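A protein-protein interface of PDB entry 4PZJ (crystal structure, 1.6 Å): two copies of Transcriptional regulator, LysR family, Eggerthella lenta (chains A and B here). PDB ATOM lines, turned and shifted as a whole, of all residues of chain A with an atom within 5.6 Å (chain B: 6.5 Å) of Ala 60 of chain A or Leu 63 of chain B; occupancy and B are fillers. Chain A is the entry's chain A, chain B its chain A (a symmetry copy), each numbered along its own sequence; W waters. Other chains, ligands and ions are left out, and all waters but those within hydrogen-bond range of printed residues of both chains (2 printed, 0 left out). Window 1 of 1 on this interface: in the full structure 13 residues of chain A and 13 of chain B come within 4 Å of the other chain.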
ATOM      1  N   MET A   1      17.506  25.046 -16.240  1.00  0.00           N
ATOM      2  CA  MET A   1      16.858  23.736 -16.576  1.00  0.00           C
ATOM      3  C   MET A   1      17.160  23.415 -18.012  1.00  0.00           C
ATOM      4  O   MET A   1      17.095  24.278 -18.900  1.00  0.00           O
ATOM      5  CB  MET A   1      15.361  23.703 -16.257  1.00  0.00           C
ATOM      6  CG  MET A   1      14.592  24.874 -16.866  1.00  0.00           C
ATOM      7  SD  MET A   1      12.807  25.112 -16.034  1.00  0.00           S
ATOM      8  CE  MET A   1      12.777  23.856 -14.536  1.00  0.00           C
ATOM      9  N   TYR A  43      13.667  20.428  -8.082  1.00  0.00           N
ATOM     10  CA  TYR A  43      12.862  21.523  -7.555  1.00  0.00           C
ATOM     11  C   TYR A  43      12.021  21.160  -6.343  1.00  0.00           C
ATOM     12  O   TYR A  43      11.547  22.028  -5.640  1.00  0.00           O
ATOM     13  CB  TYR A  43      12.004  22.167  -8.670  1.00  0.00           C
ATOM     14  CG  TYR A  43      12.930  22.855  -9.639  1.00  0.00           C
ATOM     15  CD1 TYR A  43      13.372  24.144  -9.395  1.00  0.00           C
ATOM     16  CD2 TYR A  43      13.392  22.201 -10.777  1.00  0.00           C
ATOM     17  CE1 TYR A  43      14.260  24.759 -10.255  1.00  0.00           C
ATOM     18  CE2 TYR A  43      14.282  22.820 -11.650  1.00  0.00           C
ATOM     19  CZ  TYR A  43      14.680  24.112 -11.385  1.00  0.00           C
ATOM     20  OH  TYR A  43      15.577  24.749 -12.218  1.00  0.00           O
ATOM     21  N   VAL A  45       9.144  19.636  -6.148  1.00  0.00           N
ATOM     22  CA  VAL A  45       7.683  19.741  -6.300  1.00  0.00           C
ATOM     23  C   VAL A  45       7.230  18.780  -7.397  1.00  0.00           C
ATOM     24  O   VAL A  45       7.962  18.591  -8.407  1.00  0.00           O
ATOM     25  CB  VAL A  45       7.221  21.178  -6.651  1.00  0.00           C
ATOM     26  CG1 VAL A  45       7.470  22.127  -5.484  1.00  0.00           C
ATOM     27  CG2 VAL A  45       7.893  21.684  -7.921  1.00  0.00           C
ATOM     28  N   PRO A  46       6.061  18.160  -7.248  1.00  0.00           N
ATOM     29  CA  PRO A  46       5.551  17.300  -8.274  1.00  0.00           C
ATOM     30  C   PRO A  46       4.940  18.148  -9.402  1.00  0.00           C
ATOM     31  O   PRO A  46       4.369  19.209  -9.124  1.00  0.00           O
ATOM     32  CB  PRO A  46       4.410  16.563  -7.589  1.00  0.00           C
ATOM     33  CG  PRO A  46       3.867  17.572  -6.657  1.00  0.00           C
ATOM     34  CD  PRO A  46       5.056  18.362  -6.172  1.00  0.00           C
ATOM     35  N   LEU A  47       5.053  17.649 -10.615  1.00  0.00           N
ATOM     36  CA  LEU A  47       4.514  18.353 -11.789  1.00  0.00           C
ATOM     37  C   LEU A  47       3.264  17.668 -12.320  1.00  0.00           C
ATOM     38  O   LEU A  47       2.445  18.283 -13.010  1.00  0.00           O
ATOM     39  CB  LEU A  47       5.613  18.401 -12.860  1.00  0.00           C
ATOM     40  CG  LEU A  47       6.792  19.261 -12.475  1.00  0.00           C
ATOM     41  CD1 LEU A  47       7.900  19.056 -13.517  1.00  0.00           C
ATOM     42  CD2 LEU A  47       6.528  20.748 -12.267  1.00  0.00           C
ATOM     43  N   THR A  58      -0.253  19.219 -11.880  1.00  0.00           N
ATOM     44  CA  THR A  58      -0.288  19.835 -10.567  1.00  0.00           C
ATOM     45  C   THR A  58      -0.257  21.367 -10.593  1.00  0.00           C
ATOM     46  O   THR A  58      -0.111  21.981 -11.660  1.00  0.00           O
ATOM     47  CB  THR A  58       0.886  19.379  -9.706  1.00  0.00           C
ATOM     48  OG1 THR A  58       2.086  19.938 -10.268  1.00  0.00           O
ATOM     49  CG2 THR A  58       0.974  17.915  -9.657  1.00  0.00           C
ATOM     50  N   ASP A  59      -0.454  22.001  -9.431  1.00  0.00           N
ATOM     51  CA  ASP A  59      -0.343  23.452  -9.347  1.00  0.00           C
ATOM     52  C   ASP A  59       1.034  23.913  -9.813  1.00  0.00           C
ATOM     53  O   ASP A  59       1.128  24.872 -10.555  1.00  0.00           O
ATOM     54  CB  ASP A  59      -0.621  23.940  -7.937  1.00  0.00           C
ATOM     55  CG  ASP A  59      -2.081  23.765  -7.530  1.00  0.00           C
ATOM     56  OD1 ASP A  59      -2.950  23.594  -8.393  1.00  0.00           O
ATOM     57  OD2 ASP A  59      -2.350  23.843  -6.321  1.00  0.00           O
ATOM     58  N   ALA A  60       2.100  23.240  -9.397  1.00  0.00           N
ATOM     59  CA  ALA A  60       3.469  23.606  -9.862  1.00  0.00           C
ATOM     60  C   ALA A  60       3.626  23.364 -11.358  1.00  0.00           C
ATOM     61  O   ALA A  60       4.313  24.149 -12.058  1.00  0.00           O
ATOM     62  CB  ALA A  60       4.519  22.808  -9.112  1.00  0.00           C
ATOM     63  N   GLY A  61       3.007  22.306 -11.870  1.00  0.00           N
ATOM     64  CA  GLY A  61       3.006  21.995 -13.312  1.00  0.00           C
ATOM     65  C   GLY A  61       2.398  23.153 -14.106  1.00  0.00           C
ATOM     66  O   GLY A  61       2.916  23.562 -15.121  1.00  0.00           O
ATOM     67  N   ALA A  62       1.269  23.686 -13.633  1.00  0.00           N
ATOM     68  CA  ALA A  62       0.636  24.812 -14.315  1.00  0.00           C
ATOM     69  C   ALA A  62       1.481  26.091 -14.260  1.00  0.00           C
ATOM     70  O   ALA A  62       1.513  26.868 -15.223  1.00  0.00           O
ATOM     71  CB  ALA A  62      -0.750  25.026 -13.701  1.00  0.00           C
ATOM     72  N   LEU A  63       2.211  26.323 -13.163  1.00  0.00           N
ATOM     73  CA  LEU A  63       3.031  27.471 -12.993  1.00  0.00           C
ATOM     74  C   LEU A  63       4.207  27.337 -13.977  1.00  0.00           C
ATOM     75  O   LEU A  63       4.521  28.279 -14.699  1.00  0.00           O
ATOM     76  CB  LEU A  63       3.550  27.528 -11.559  1.00  0.00           C
ATOM     77  CG  LEU A  63       4.478  28.687 -11.190  1.00  0.00           C
ATOM     78  CD1 LEU A  63       3.804  30.032 -11.214  1.00  0.00           C
ATOM     79  CD2 LEU A  63       5.145  28.412  -9.829  1.00  0.00           C
ATOM     80  N   LEU A  64       4.771  26.137 -14.049  1.00  0.00           N
ATOM     81  CA  LEU A  64       5.889  25.879 -14.988  1.00  0.00           C
ATOM     82  C   LEU A  64       5.417  26.100 -16.426  1.00  0.00           C
ATOM     83  O   LEU A  64       6.112  26.761 -17.231  1.00  0.00           O
ATOM     84  CB  LEU A  64       6.443  24.455 -14.809  1.00  0.00           C
ATOM     85  CG  LEU A  64       7.653  24.096 -15.712  1.00  0.00           C
ATOM     86  CD1 LEU A  64       8.792  25.076 -15.565  1.00  0.00           C
ATOM     87  CD2 LEU A  64       8.100  22.695 -15.387  1.00  0.00           C
ATOM     88  N   ARG A  65       4.268  25.519 -16.766  1.00  0.00           N
ATOM     89  CA  ARG A  65       3.696  25.673 -18.112  1.00  0.00           C
ATOM     90  C   ARG A  65       3.598  27.127 -18.487  1.00  0.00           C
ATOM     91  O   ARG A  65       4.068  27.535 -19.550  1.00  0.00           O
ATOM     92  CB  ARG A  65       2.295  25.036 -18.196  1.00  0.00           C
ATOM     93  CG  ARG A  65       1.566  25.237 -19.555  1.00  0.00           C
ATOM     94  CD  ARG A  65       0.086  24.951 -19.360  1.00  0.00           C
ATOM     95  NE  ARG A  65      -0.449  25.929 -18.466  1.00  0.00           N
ATOM     96  CZ  ARG A  65      -1.464  25.756 -17.629  1.00  0.00           C
ATOM     97  NH1 ARG A  65      -1.803  26.752 -16.841  1.00  0.00           N
ATOM     98  NH2 ARG A  65      -2.056  24.587 -17.495  1.00  0.00           N
ATOM     99  N   TYR B  43      -2.056  30.450  -8.869  1.00  0.00           N
ATOM    100  CA  TYR B  43      -1.391  29.165  -9.036  1.00  0.00           C
ATOM    101  C   TYR B  43      -1.490  28.242  -7.833  1.00  0.00           C
ATOM    102  O   TYR B  43      -1.247  27.059  -7.944  1.00  0.00           O
ATOM    103  CB  TYR B  43       0.076  29.354  -9.488  1.00  0.00           C
ATOM    104  CG  TYR B  43       0.070  29.924 -10.882  1.00  0.00           C
ATOM    105  CD1 TYR B  43      -0.038  29.091 -11.982  1.00  0.00           C
ATOM    106  CD2 TYR B  43       0.135  31.298 -11.096  1.00  0.00           C
ATOM    107  CE1 TYR B  43      -0.094  29.613 -13.259  1.00  0.00           C
ATOM    108  CE2 TYR B  43       0.086  31.828 -12.382  1.00  0.00           C
ATOM    109  CZ  TYR B  43       0.001  30.964 -13.452  1.00  0.00           C
ATOM    110  OH  TYR B  43      -0.071  31.456 -14.740  1.00  0.00           O
ATOM    111  N   VAL B  45       0.233  28.189  -5.065  1.00  0.00           N
ATOM    112  CA  VAL B  45       1.498  27.817  -4.410  1.00  0.00           C
ATOM    113  C   VAL B  45       2.173  29.081  -3.883  1.00  0.00           C
ATOM    114  O   VAL B  45       2.089  30.156  -4.538  1.00  0.00           O
ATOM    115  CB  VAL B  45       2.468  27.074  -5.364  1.00  0.00           C
ATOM    116  CG1 VAL B  45       1.913  25.705  -5.743  1.00  0.00           C
ATOM    117  CG2 VAL B  45       2.773  27.903  -6.604  1.00  0.00           C
ATOM    118  N   LEU B  57      12.987  32.019  -0.583  1.00  0.00           N
ATOM    119  CA  LEU B  57      12.363  31.691  -1.838  1.00  0.00           C
ATOM    120  C   LEU B  57      11.914  30.243  -1.691  1.00  0.00           C
ATOM    121  O   LEU B  57      12.714  29.342  -1.342  1.00  0.00           O
ATOM    122  CB  LEU B  57      13.353  31.811  -2.983  1.00  0.00           C
ATOM    123  CG  LEU B  57      12.807  31.579  -4.362  1.00  0.00           C
ATOM    124  CD1 LEU B  57      11.930  32.760  -4.799  1.00  0.00           C
ATOM    125  CD2 LEU B  57      13.952  31.438  -5.358  1.00  0.00           C
ATOM    126  N   THR B  58      10.635  29.980  -1.914  1.00  0.00           N
ATOM    127  CA  THR B  58      10.127  28.623  -1.835  1.00  0.00           C
ATOM    128  C   THR B  58      10.559  27.724  -2.998  1.00  0.00           C
ATOM    129  O   THR B  58      11.201  28.186  -3.953  1.00  0.00           O
ATOM    130  CB  THR B  58       8.603  28.599  -1.795  1.00  0.00           C
ATOM    131  OG1 THR B  58       8.123  29.024  -3.081  1.00  0.00           O
ATOM    132  CG2 THR B  58       8.083  29.474  -0.737  1.00  0.00           C
ATOM    133  N   ASP B  59      10.268  26.421  -2.905  1.00  0.00           N
ATOM    134  CA  ASP B  59      10.554  25.512  -4.008  1.00  0.00           C
ATOM    135  C   ASP B  59       9.853  25.978  -5.281  1.00  0.00           C
ATOM    136  O   ASP B  59      10.459  25.975  -6.336  1.00  0.00           O
ATOM    137  CB  ASP B  59      10.149  24.091  -3.663  1.00  0.00           C
ATOM    138  CG  ASP B  59      11.029  23.473  -2.582  1.00  0.00           C
ATOM    139  OD1 ASP B  59      12.134  23.967  -2.323  1.00  0.00           O
ATOM    140  OD2 ASP B  59      10.608  22.451  -2.017  1.00  0.00           O
ATOM    141  N   ALA B  60       8.593  26.384  -5.196  1.00  0.00           N
ATOM    142  CA  ALA B  60       7.871  26.902  -6.394  1.00  0.00           C
ATOM    143  C   ALA B  60       8.489  28.204  -6.888  1.00  0.00           C
ATOM    144  O   ALA B  60       8.554  28.447  -8.119  1.00  0.00           O
ATOM    145  CB  ALA B  60       6.405  27.133  -6.076  1.00  0.00           C
ATOM    146  N   GLY B  61       8.950  29.046  -5.969  1.00  0.00           N
ATOM    147  CA  GLY B  61       9.643  30.304  -6.306  1.00  0.00           C
ATOM    148  C   GLY B  61      10.887  30.016  -7.148  1.00  0.00           C
ATOM    149  O   GLY B  61      11.148  30.671  -8.132  1.00  0.00           O
ATOM    150  N   ALA B  62      11.675  29.016  -6.744  1.00  0.00           N
ATOM    151  CA  ALA B  62      12.870  28.659  -7.505  1.00  0.00           C
ATOM    152  C   ALA B  62      12.543  28.088  -8.891  1.00  0.00           C
ATOM    153  O   ALA B  62      13.265  28.341  -9.864  1.00  0.00           O
ATOM    154  CB  ALA B  62      13.692  27.673  -6.670  1.00  0.00           C
ATOM    155  N   LEU B  63      11.439  27.344  -9.027  1.00  0.00           N
ATOM    156  CA  LEU B  63      11.031  26.761 -10.256  1.00  0.00           C
ATOM    157  C   LEU B  63      10.599  27.911 -11.183  1.00  0.00           C
ATOM    158  O   LEU B  63      11.015  27.968 -12.337  1.00  0.00           O
ATOM    159  CB  LEU B  63       9.861  25.812 -10.016  1.00  0.00           C
ATOM    160  CG  LEU B  63       9.263  25.105 -11.234  1.00  0.00           C
ATOM    161  CD1 LEU B  63      10.196  24.114 -11.876  1.00  0.00           C
ATOM    162  CD2 LEU B  63       7.919  24.454 -10.856  1.00  0.00           C
ATOM    163  N   LEU B  64       9.847  28.853 -10.627  1.00  0.00           N
ATOM    164  CA  LEU B  64       9.400  30.030 -11.412  1.00  0.00           C
ATOM    165  C   LEU B  64      10.617  30.826 -11.886  1.00  0.00           C
ATOM    166  O   LEU B  64      10.696  31.224 -13.071  1.00  0.00           O
ATOM    167  CB  LEU B  64       8.455  30.918 -10.585  1.00  0.00           C
ATOM    168  CG  LEU B  64       7.887  32.155 -11.331  1.00  0.00           C
ATOM    169  CD1 LEU B  64       7.191  31.782 -12.619  1.00  0.00           C
ATOM    170  CD2 LEU B  64       6.953  32.891 -10.407  1.00  0.00           C
ATOM    171  N   ARG B  65      11.539  31.098 -10.965  1.00  0.00           N
ATOM    172  CA  ARG B  65      12.766  31.838 -11.300  1.00  0.00           C
ATOM    173  C   ARG B  65      13.466  31.208 -12.473  1.00  0.00           C
ATOM    174  O   ARG B  65      13.791  31.886 -13.449  1.00  0.00           O
ATOM    175  CB  ARG B  65      13.733  31.881 -10.100  1.00  0.00           C
ATOM    176  CG  ARG B  65      15.103  32.557 -10.389  1.00  0.00           C
ATOM    177  CD  ARG B  65      16.082  32.159  -9.297  1.00  0.00           C
ATOM    178  NE  ARG B  65      16.301  30.748  -9.380  1.00  0.00           N
ATOM    179  CZ  ARG B  65      16.598  29.939  -8.371  1.00  0.00           C
ATOM    180  NH1 ARG B  65      16.725  28.654  -8.616  1.00  0.00           N
ATOM    181  NH2 ARG B  65      16.654  30.376  -7.130  1.00  0.00           N
ATOM    182  N   ASP B  66      13.780  29.918 -12.360  1.00  0.00           N
ATOM    183  CA  ASP B  66      14.511  29.253 -13.441  1.00  0.00           C
ATOM    184  C   ASP B  66      13.716  29.139 -14.740  1.00  0.00           C
ATOM    185  O   ASP B  66      14.264  29.212 -15.817  1.00  0.00           O
ATOM    186  CB  ASP B  66      15.037  27.897 -12.967  1.00  0.00           C
ATOM    187  CG  ASP B  66      16.104  28.016 -11.906  1.00  0.00           C
ATOM    188  OD1 ASP B  66      16.645  29.119 -11.653  1.00  0.00           O
ATOM    189  OD2 ASP B  66      16.437  26.963 -11.315  1.00  0.00           O
ATOM    190  N   ALA B  67      12.400  28.953 -14.655  1.00  0.00           N
ATOM    191  CA  ALA B  67      11.588  28.816 -15.864  1.00  0.00           C
ATOM    192  C   ALA B  67      11.551  30.109 -16.638  1.00  0.00           C
ATOM    193  O   ALA B  67      11.527  30.097 -17.863  1.00  0.00           O
ATOM    194  CB  ALA B  67      10.167  28.425 -15.487  1.00  0.00           C
ATOM    195  N   LEU B  68      11.569  31.218 -15.914  1.00  0.00           N
ATOM    196  CA  LEU B  68      11.508  32.546 -16.539  1.00  0.00           C
ATOM    197  C   LEU B  68      12.810  32.901 -17.236  1.00  0.00           C
ATOM    198  O   LEU B  68      12.809  33.726 -18.138  1.00  0.00           O
ATOM    199  CB  LEU B  68      11.117  33.631 -15.548  1.00  0.00           C
ATOM    200  CG  LEU B  68       9.673  33.567 -15.036  1.00  0.00           C
ATOM    201  CD1 LEU B  68       9.464  34.482 -13.854  1.00  0.00           C
ATOM    202  CD2 LEU B  68       8.738  33.942 -16.167  1.00  0.00           C
HETATM  203  O   HOH W   1      12.793  24.379  -6.050  1.00  0.00           O
HETATM  204  O   HOH W   2      -1.328  26.300 -10.525  1.00  0.00           O
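Water W2 lies within hydrogen-bond range of the backbone carbonyl oxygen (O) of Tyr 43 of chain B (2.7 Å) and the backbone carbonyl oxygen (O) of Asp 59 of chain A (2.8 Å).
Water W1 lies within hydrogen-bond range of O of Tyr 43 of chain A and O of Asp 59 of chain B.
Leu 47 of chain A touches none of the printed residues of chain B.
Of chain B, only Leu 63 (3.8 Å) comes within 4 Å of Ala 60 of chain A.
Leu 57 of chain B touches none of the printed residues of chain A.
Of the printed residues of chain A, Ala 60 of chain B touches Leu 63.
Leu 63 of chain B touches three residues of chain A.
Of the printed residues of chain A, Ala 67 of chain B touches Met 1 and Leu 64.
The nearest residue of chain B that does not touch Ala 60 of chain A is Val 45 of chain B (4.4 Å).
The nearest printed residue of chain A that does not touch Leu 63 of chain B is Val 45 of chain A (4.04 Å).
Of the 13 printed residues of chain A, 8 touch a printed residue of chain B.
Hydrophobic or aromatic side chains of chain A that line the printed part of chain B: Met 1, Tyr 43, Val 45, Leu 63 and Leu 64.
Of the 14 printed residues of chain B, 8 touch a printed residue of chain A.
Hydrophobic or aromatic side chains of chain B within 4 Å of the printed part of chain A: Tyr 43, Val 45, Leu 63 and Ala 67.
Among the printed residues, 14 pairs touch across the chains.
Among the printed residues, no Asp or Glu carboxylate lies within 4 Å of a Lys or Arg side-chain nitrogen of the other chain.
OH of Tyr 43 of chain A sits at hydrogen-bond distance from OD2 of Asp 66 of chain B, 2.5 Å away.
The guanidinium group of Arg 65 of chain B is in salt-bridge range of the side-chain carboxylate of Asp 66 of chain B (2.8 Å).
The backbone NH (N) of Ala 60 of chain B lies close to the side-chain hydroxyl (OG1) of Thr 58 of chain B, 3.4 Å away.
The side-chain hydroxyl (OG1) of Thr 58 of chain A lies close to the backbone NH (N) of Ala 60 of chain A (3.4 Å).
Tyr 43 of chain A touches Ala 62 of chain B, and with the chains exchanged Ala 62 of chain A touches Tyr 43 of chain B.
Tyr 43 of chain A touches Leu 63 of chain B, and with the chains exchanged Leu 63 of chain A touches Tyr 43 of chain B.
Val 45 of chain A touches Asp 59 of chain B, and with the chains exchanged Asp 59 of chain A touches Val 45 of chain B.
Ala 60 of chain A touches Leu 63 of chain B, and with the chains exchanged Leu 63 of chain A touches Ala 60 of chain B.
Of the 14 pairs that touch across the chains among the printed residues, 10 have their exchanged pair printed and touching as well.
Among the printed residues, pairs that only touch across the chains: Met 1 of chain A with Leu 63 of chain B, Met 1 of chain A with Ala 67 of chain B, Tyr 43 of chain A with Asp 59 of chain B, Tyr 43 of chain A with Ala 62 of chain B, Tyr 43 of chain A with Leu 63 of chain B, Val 45 of chain A with Asp 59 of chain B, Asp 59 of chain A with Tyr 43 of chain B, Asp 59 of chain A with Val 45 of chain B, Ala 60 of chain A with Leu 63 of chain B, Ala 62 of chain A with Tyr 43 of chain B, Leu 63 of chain A with Tyr 43 of chain B, Leu 63 of chain A with Ala 60 of chain B and Leu 64 of chain A with Ala 67 of chain B.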
